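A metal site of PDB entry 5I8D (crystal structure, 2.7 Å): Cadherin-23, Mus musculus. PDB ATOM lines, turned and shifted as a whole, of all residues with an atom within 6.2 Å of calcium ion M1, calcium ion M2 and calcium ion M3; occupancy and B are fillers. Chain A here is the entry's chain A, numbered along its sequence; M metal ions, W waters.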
ATOM      1  N   GLU A  23      -5.852  -7.041  25.901  1.00  0.00           N
ATOM      2  CA  GLU A  23      -6.281  -8.264  25.202  1.00  0.00           C
ATOM      3  C   GLU A  23      -6.585  -9.374  26.243  1.00  0.00           C
ATOM      4  O   GLU A  23      -6.188  -9.273  27.405  1.00  0.00           O
ATOM      5  CB  GLU A  23      -5.233  -8.732  24.165  1.00  0.00           C
ATOM      6  CG  GLU A  23      -3.874  -9.195  24.726  1.00  0.00           C
ATOM      7  CD  GLU A  23      -2.960  -9.854  23.688  1.00  0.00           C
ATOM      8  OE1 GLU A  23      -1.737  -9.885  23.950  1.00  0.00           O
ATOM      9  OE2 GLU A  23      -3.448 -10.342  22.629  1.00  0.00           O
ATOM     10  N   ASN A  24      -7.317 -10.400  25.807  1.00  0.00           N
ATOM     11  CA  ASN A  24      -7.697 -11.542  26.669  1.00  0.00           C
ATOM     12  C   ASN A  24      -8.482 -11.085  27.916  1.00  0.00           C
ATOM     13  O   ASN A  24      -8.475 -11.774  28.937  1.00  0.00           O
ATOM     14  CB  ASN A  24      -6.473 -12.366  27.122  1.00  0.00           C
ATOM     15  CG  ASN A  24      -5.523 -12.707  25.982  1.00  0.00           C
ATOM     16  OD1 ASN A  24      -5.940 -13.066  24.876  1.00  0.00           O
ATOM     17  ND2 ASN A  24      -4.211 -12.609  26.262  1.00  0.00           N
ATOM     18  N   ILE A  80     -10.696 -11.230  22.581  1.00  0.00           N
ATOM     19  CA  ILE A  80      -9.960 -10.084  22.009  1.00  0.00           C
ATOM     20  C   ILE A  80      -8.461 -10.405  21.998  1.00  0.00           C
ATOM     21  O   ILE A  80      -7.820 -10.401  23.050  1.00  0.00           O
ATOM     22  CB  ILE A  80     -10.214  -8.764  22.797  1.00  0.00           C
ATOM     23  CG1 ILE A  80     -11.714  -8.430  22.804  1.00  0.00           C
ATOM     24  CG2 ILE A  80      -9.404  -7.616  22.182  1.00  0.00           C
ATOM     25  CD1 ILE A  80     -12.084  -7.259  23.693  1.00  0.00           C
ATOM     26  N   ASP A  81      -7.918 -10.661  20.796  1.00  0.00           N
ATOM     27  CA  ASP A  81      -6.504 -11.084  20.599  1.00  0.00           C
ATOM     28  C   ASP A  81      -5.705 -10.062  19.763  1.00  0.00           C
ATOM     29  O   ASP A  81      -5.823 -10.020  18.511  1.00  0.00           O
ATOM     30  CB  ASP A  81      -6.467 -12.468  19.932  1.00  0.00           C
ATOM     31  CG  ASP A  81      -5.119 -12.790  19.280  1.00  0.00           C
ATOM     32  OD1 ASP A  81      -4.063 -12.514  19.897  1.00  0.00           O
ATOM     33  OD2 ASP A  81      -5.116 -13.322  18.154  1.00  0.00           O
ATOM     34  N   ARG A  82      -4.859  -9.295  20.441  1.00  0.00           N
ATOM     35  CA  ARG A  82      -4.034  -8.266  19.779  1.00  0.00           C
ATOM     36  C   ARG A  82      -3.364  -8.760  18.476  1.00  0.00           C
ATOM     37  O   ARG A  82      -3.475  -8.116  17.418  1.00  0.00           O
ATOM     38  CB  ARG A  82      -2.977  -7.719  20.740  1.00  0.00           C
ATOM     39  CG  ARG A  82      -2.384  -6.392  20.303  1.00  0.00           C
ATOM     40  CD  ARG A  82      -1.108  -6.082  21.067  1.00  0.00           C
ATOM     41  NE  ARG A  82       0.009  -6.922  20.631  1.00  0.00           N
ATOM     42  CZ  ARG A  82       0.800  -6.702  19.580  1.00  0.00           C
ATOM     43  NH1 ARG A  82       1.786  -7.561  19.301  1.00  0.00           N
ATOM     44  NH2 ARG A  82       0.628  -5.624  18.779  1.00  0.00           N
ATOM     45  N   GLU A  83      -2.775  -9.950  18.561  1.00  0.00           N
ATOM     46  CA  GLU A  83      -2.088 -10.585  17.438  1.00  0.00           C
ATOM     47  C   GLU A  83      -2.959 -10.864  16.189  1.00  0.00           C
ATOM     48  O   GLU A  83      -2.399 -11.261  15.167  1.00  0.00           O
ATOM     49  CB  GLU A  83      -1.444 -11.915  17.883  1.00  0.00           C
ATOM     50  CG  GLU A  83      -0.170 -11.742  18.685  1.00  0.00           C
ATOM     51  CD  GLU A  83      -0.404 -11.119  20.044  1.00  0.00           C
ATOM     52  OE1 GLU A  83      -1.159 -11.696  20.869  1.00  0.00           O
ATOM     53  OE2 GLU A  83       0.175 -10.044  20.305  1.00  0.00           O
ATOM     54  N   ASP A 114      -1.205  -4.693  24.783  1.00  0.00           N
ATOM     55  CA  ASP A 114      -0.494  -5.990  24.671  1.00  0.00           C
ATOM     56  C   ASP A 114      -0.343  -6.724  25.991  1.00  0.00           C
ATOM     57  O   ASP A 114      -0.002  -6.139  27.022  1.00  0.00           O
ATOM     58  CB  ASP A 114       0.904  -5.819  24.040  1.00  0.00           C
ATOM     59  CG  ASP A 114       1.580  -7.173  23.715  1.00  0.00           C
ATOM     60  OD1 ASP A 114       0.928  -8.061  23.103  1.00  0.00           O
ATOM     61  OD2 ASP A 114       2.767  -7.363  24.061  1.00  0.00           O
ATOM     62  N   ASP A 115      -0.573  -8.042  25.904  1.00  0.00           N
ATOM     63  CA  ASP A 115      -0.355  -8.983  27.000  1.00  0.00           C
ATOM     64  C   ASP A 115       0.696  -9.980  26.525  1.00  0.00           C
ATOM     65  O   ASP A 115       0.673 -10.412  25.383  1.00  0.00           O
ATOM     66  CB  ASP A 115      -1.666  -9.695  27.316  1.00  0.00           C
ATOM     67  CG  ASP A 115      -1.575 -10.646  28.484  1.00  0.00           C
ATOM     68  OD1 ASP A 115      -0.740 -10.412  29.399  1.00  0.00           O
ATOM     69  OD2 ASP A 115      -2.373 -11.626  28.484  1.00  0.00           O
ATOM     70  N   ASN A 116       1.617 -10.350  27.409  1.00  0.00           N
ATOM     71  CA  ASN A 116       2.691 -11.267  27.059  1.00  0.00           C
ATOM     72  C   ASN A 116       2.159 -12.699  27.019  1.00  0.00           C
ATOM     73  O   ASN A 116       2.376 -13.477  27.953  1.00  0.00           O
ATOM     74  CB  ASN A 116       3.847 -11.124  28.051  1.00  0.00           C
ATOM     75  CG  ASN A 116       5.098 -11.845  27.600  1.00  0.00           C
ATOM     76  OD1 ASN A 116       5.383 -11.942  26.406  1.00  0.00           O
ATOM     77  ND2 ASN A 116       5.862 -12.362  28.550  1.00  0.00           N
ATOM     78  N   ASP A 117       1.452 -13.026  25.924  1.00  0.00           N
ATOM     79  CA  ASP A 117       0.747 -14.314  25.794  1.00  0.00           C
ATOM     80  C   ASP A 117       1.270 -15.245  24.692  1.00  0.00           C
ATOM     81  O   ASP A 117       0.631 -16.249  24.360  1.00  0.00           O
ATOM     82  CB  ASP A 117      -0.774 -14.090  25.649  1.00  0.00           C
ATOM     83  CG  ASP A 117      -1.165 -13.417  24.349  1.00  0.00           C
ATOM     84  OD1 ASP A 117      -0.444 -12.547  23.823  1.00  0.00           O
ATOM     85  OD2 ASP A 117      -2.253 -13.754  23.843  1.00  0.00           O
ATOM     86  N   ASN A 118       2.450 -14.903  24.151  1.00  0.00           N
ATOM     87  CA  ASN A 118       3.144 -15.708  23.122  1.00  0.00           C
ATOM     88  C   ASN A 118       4.550 -16.013  23.592  1.00  0.00           C
ATOM     89  O   ASN A 118       5.268 -15.111  24.018  1.00  0.00           O
ATOM     90  CB  ASN A 118       3.224 -14.972  21.785  1.00  0.00           C
ATOM     91  CG  ASN A 118       1.899 -14.954  21.045  1.00  0.00           C
ATOM     92  OD1 ASN A 118       1.654 -15.801  20.204  1.00  0.00           O
ATOM     93  ND2 ASN A 118       1.049 -13.985  21.352  1.00  0.00           N
ATOM     94  N   TRP A 119       4.948 -17.279  23.470  1.00  0.00           N
ATOM     95  CA  TRP A 119       6.265 -17.744  23.895  1.00  0.00           C
ATOM     96  C   TRP A 119       7.314 -17.447  22.805  1.00  0.00           C
ATOM     97  O   TRP A 119       7.028 -17.601  21.630  1.00  0.00           O
ATOM     98  CB  TRP A 119       6.253 -19.253  24.155  1.00  0.00           C
ATOM     99  CG  TRP A 119       5.650 -19.693  25.469  1.00  0.00           C
ATOM    100  CD1 TRP A 119       6.331 -20.068  26.586  1.00  0.00           C
ATOM    101  CD2 TRP A 119       4.260 -19.862  25.767  1.00  0.00           C
ATOM    102  NE1 TRP A 119       5.451 -20.431  27.573  1.00  0.00           N
ATOM    103  CE2 TRP A 119       4.178 -20.317  27.098  1.00  0.00           C
ATOM    104  CE3 TRP A 119       3.068 -19.656  25.042  1.00  0.00           C
ATOM    105  CZ2 TRP A 119       2.944 -20.579  27.728  1.00  0.00           C
ATOM    106  CZ3 TRP A 119       1.852 -19.918  25.673  1.00  0.00           C
ATOM    107  CH2 TRP A 119       1.792 -20.367  26.997  1.00  0.00           C
ATOM    108  N   PRO A 120       8.536 -17.022  23.204  1.00  0.00           N
ATOM    109  CA  PRO A 120       9.638 -17.134  22.246  1.00  0.00           C
ATOM    110  C   PRO A 120       9.720 -18.580  21.724  1.00  0.00           C
ATOM    111  O   PRO A 120       9.911 -19.501  22.521  1.00  0.00           O
ATOM    112  CB  PRO A 120      10.874 -16.797  23.096  1.00  0.00           C
ATOM    113  CG  PRO A 120      10.358 -15.921  24.186  1.00  0.00           C
ATOM    114  CD  PRO A 120       8.940 -16.334  24.450  1.00  0.00           C
ATOM    115  N   ASP A 148       8.915 -14.281  18.338  1.00  0.00           N
ATOM    116  CA  ASP A 148       7.913 -14.010  19.385  1.00  0.00           C
ATOM    117  C   ASP A 148       6.869 -13.048  18.813  1.00  0.00           C
ATOM    118  O   ASP A 148       7.203 -11.903  18.479  1.00  0.00           O
ATOM    119  CB  ASP A 148       8.614 -13.399  20.618  1.00  0.00           C
ATOM    120  CG  ASP A 148       7.681 -13.226  21.831  1.00  0.00           C
ATOM    121  OD1 ASP A 148       6.507 -12.824  21.673  1.00  0.00           O
ATOM    122  OD2 ASP A 148       8.133 -13.477  22.985  1.00  0.00           O
ATOM    123  N   GLU A 149       5.610 -13.481  18.730  1.00  0.00           N
ATOM    124  CA  GLU A 149       4.552 -12.671  18.105  1.00  0.00           C
ATOM    125  C   GLU A 149       4.065 -11.466  18.953  1.00  0.00           C
ATOM    126  O   GLU A 149       3.246 -10.686  18.484  1.00  0.00           O
ATOM    127  CB  GLU A 149       3.342 -13.538  17.724  1.00  0.00           C
ATOM    128  CG  GLU A 149       3.640 -14.792  16.906  1.00  0.00           C
ATOM    129  CD  GLU A 149       4.604 -14.571  15.751  1.00  0.00           C
ATOM    130  OE1 GLU A 149       5.773 -15.015  15.850  1.00  0.00           O
ATOM    131  OE2 GLU A 149       4.194 -13.960  14.735  1.00  0.00           O
ATOM    132  N   ASP A 150       4.542 -11.318  20.181  1.00  0.00           N
ATOM    133  CA  ASP A 150       4.217 -10.134  20.992  1.00  0.00           C
ATOM    134  C   ASP A 150       5.073  -8.928  20.568  1.00  0.00           C
ATOM    135  O   ASP A 150       6.010  -9.057  19.754  1.00  0.00           O
ATOM    136  CB  ASP A 150       4.402 -10.421  22.490  1.00  0.00           C
ATOM    137  CG  ASP A 150       3.534 -11.574  22.982  1.00  0.00           C
ATOM    138  OD1 ASP A 150       2.372 -11.722  22.516  1.00  0.00           O
ATOM    139  OD2 ASP A 150       4.032 -12.339  23.842  1.00  0.00           O
ATOM    140  N   SER A 151       4.729  -7.771  21.144  1.00  0.00           N
ATOM    141  CA  SER A 151       5.371  -6.485  20.827  1.00  0.00           C
ATOM    142  C   SER A 151       6.183  -5.971  22.023  1.00  0.00           C
ATOM    143  O   SER A 151       6.300  -6.644  23.060  1.00  0.00           O
ATOM    144  CB  SER A 151       4.303  -5.461  20.419  1.00  0.00           C
ATOM    145  OG  SER A 151       3.462  -5.130  21.519  1.00  0.00           O
ATOM    146  N   LEU A 153       8.553  -4.930  24.905  1.00  0.00           N
ATOM    147  CA  LEU A 153       9.366  -5.784  25.756  1.00  0.00           C
ATOM    148  C   LEU A 153       8.835  -7.230  25.785  1.00  0.00           C
ATOM    149  O   LEU A 153       9.593  -8.180  26.062  1.00  0.00           O
ATOM    150  CB  LEU A 153       9.440  -5.196  27.182  1.00  0.00           C
ATOM    151  CG  LEU A 153      10.118  -3.815  27.324  1.00  0.00           C
ATOM    152  CD1 LEU A 153       9.909  -3.231  28.718  1.00  0.00           C
ATOM    153  CD2 LEU A 153      11.600  -3.849  26.989  1.00  0.00           C
ATOM    154  N   ASN A 154       7.554  -7.396  25.455  1.00  0.00           N
ATOM    155  CA  ASN A 154       6.945  -8.730  25.401  1.00  0.00           C
ATOM    156  C   ASN A 154       7.446  -9.560  24.226  1.00  0.00           C
ATOM    157  O   ASN A 154       7.349 -10.790  24.257  1.00  0.00           O
ATOM    158  CB  ASN A 154       5.417  -8.639  25.372  1.00  0.00           C
ATOM    159  CG  ASN A 154       4.861  -7.924  26.589  1.00  0.00           C
ATOM    160  OD1 ASN A 154       5.551  -7.663  27.577  1.00  0.00           O
ATOM    161  ND2 ASN A 154       3.569  -7.610  26.538  1.00  0.00           N
ATOM    162  N   GLY A 155       7.977  -8.890  23.185  1.00  0.00           N
ATOM    163  CA  GLY A 155       8.601  -9.553  22.028  1.00  0.00           C
ATOM    164  C   GLY A 155      10.116  -9.450  21.880  1.00  0.00           C
ATOM    165  O   GLY A 155      10.676 -10.005  20.941  1.00  0.00           O
ATOM    166  N   LEU A 157      13.925 -10.223  22.777  1.00  0.00           N
ATOM    167  CA  LEU A 157      14.509 -11.472  23.291  1.00  0.00           C
ATOM    168  C   LEU A 157      15.977 -11.340  23.727  1.00  0.00           C
ATOM    169  O   LEU A 157      16.802 -10.781  22.998  1.00  0.00           O
ATOM    170  CB  LEU A 157      14.384 -12.575  22.229  1.00  0.00           C
ATOM    171  CG  LEU A 157      13.000 -12.683  21.566  1.00  0.00           C
ATOM    172  CD1 LEU A 157      12.943 -13.751  20.467  1.00  0.00           C
ATOM    173  CD2 LEU A 157      11.926 -12.916  22.626  1.00  0.00           C
ATOM    174  N   ASP A 201      11.942 -13.585  26.690  1.00  0.00           N
ATOM    175  CA  ASP A 201      11.393 -12.228  26.450  1.00  0.00           C
ATOM    176  C   ASP A 201      11.433 -11.334  27.702  1.00  0.00           C
ATOM    177  O   ASP A 201      11.827 -11.791  28.778  1.00  0.00           O
ATOM    178  CB  ASP A 201       9.989 -12.275  25.792  1.00  0.00           C
ATOM    179  CG  ASP A 201       8.874 -12.709  26.747  1.00  0.00           C
ATOM    180  OD1 ASP A 201       8.979 -12.500  27.972  1.00  0.00           O
ATOM    181  OD2 ASP A 201       7.861 -13.245  26.242  1.00  0.00           O
ATOM    182  N   LEU A 207       8.550 -14.890  29.525  1.00  0.00           N
ATOM    183  CA  LEU A 207       8.390 -16.218  28.908  1.00  0.00           C
ATOM    184  C   LEU A 207       9.651 -16.579  28.128  1.00  0.00           C
ATOM    185  O   LEU A 207      10.307 -15.703  27.517  1.00  0.00           O
ATOM    186  CB  LEU A 207       7.169 -16.294  27.967  1.00  0.00           C
ATOM    187  CG  LEU A 207       5.751 -16.165  28.559  1.00  0.00           C
ATOM    188  CD1 LEU A 207       4.690 -16.254  27.475  1.00  0.00           C
ATOM    189  CD2 LEU A 207       5.498 -17.228  29.623  1.00  0.00           C
HETATM  190 CA    CA M   1      -3.173 -12.722  22.035  1.00  0.00          CA
HETATM  191 CA    CA M   2       0.244 -10.489  22.884  1.00  0.00          CA
HETATM  192 CA    CA M   3       6.255 -13.065  24.537  1.00  0.00          CA
HETATM  193  O   HOH W   1      -2.012 -14.356  21.002  1.00  0.00           O
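Six residues have an atom within 4 Å of calcium ion M3: Asn 116, Asn 118, Asp 148, Asp 150, Asn 154 and Asp 201.
The nearest printed residue that does not touch calcium ion M3 is Pro 120 (4.2 Å).
Calcium ion M1 is bound by water W1 (2.3 Å).
The side-chain carboxylate (OD2) of Asp 117 binds calcium ion M1, at 2.3 Å.
OD1 of Asp 81 is bound to calcium ion M1, 2.3 Å away.
The side-chain carboxylate (OE2) of Glu 23 is bound to calcium ion M1 (2.5 Å).
Calcium ion M1 is bound by the side-chain carboxylate (OE1) of Glu 83, at 2.5 Å.
Residues that only touch calcium ion M1: Asn 24 (3.98 Å).
Five residues have an atom within 4 Å of calcium ion M1: Glu 23, Asn 24, Asp 81, Glu 83 and Asp 117.
The side-chain amide nitrogen (ND2) of Asn 118 lies close to the side-chain carboxylate (OE1) of Glu 83 (3.2 Å).
The side-chain amide nitrogen of Asn 118 lies close to the side-chain carboxylate of Asp 117 (3.2 Å).
The side-chain carboxylate (OD2) of Asp 117 sits close to the side-chain amide nitrogen (ND2) of Asn 24, at 3.3 Å.
The backbone NH (N) of Asp 201 sits at hydrogen-bond distance from the backbone carbonyl oxygen (O) of Leu 207, 2.8 Å away.
NH1 of Arg 82 lies close to OE2 of Glu 83, 3.1 Å away.
NE of Arg 82 sits close to OD1 of Asp 114 (2.9 Å).
The backbone NH of Arg 82 lies close to the side-chain carboxylate of Glu 23 (2.8 Å).
OG of Ser 151 sits at hydrogen-bond distance from OD2 of Asp 114 (3.5 Å).
Seven residues have an atom within 4 Å of calcium ion M2: Glu 23, Glu 83, Asp 114, Asp 115, Asp 117, Asn 118 and Asp 150.
Calcium ion M3 is bound by O of Asn 118 (2.3 Å).
Calcium ion M3 is bound by the side-chain amide oxygen (OD1) of Asn 116, 2.3 Å away.
OD2 of Asp 201 binds calcium ion M3 (2.3 Å).
The side-chain carboxylate (OD2) of Asp 150 is bound to calcium ion M3, at 2.4 Å.
Calcium ion M3 is bound by OD2 of Asp 148 (2.5 Å).
Calcium ion M3 is bound by O of Asn 154, at 2.5 Å.
The side-chain carboxylate (OD1) of Asp 148 binds calcium ion M3, at 2.9 Å.
Calcium ion M2 is bound by OE1 of Glu 23 (2.3 Å), OD1 of Asp 117 (2.4 Å), OD1 of Asp 150 (2.5 Å), OD1 of Asp 114 (2.5 Å), O of Asp 115 (2.5 Å), OE2 of Glu 83 (2.6 Å) and OE1 of Glu 83 (2.7 Å).
Calcium ion M2 has seven donor atoms within binding distance.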
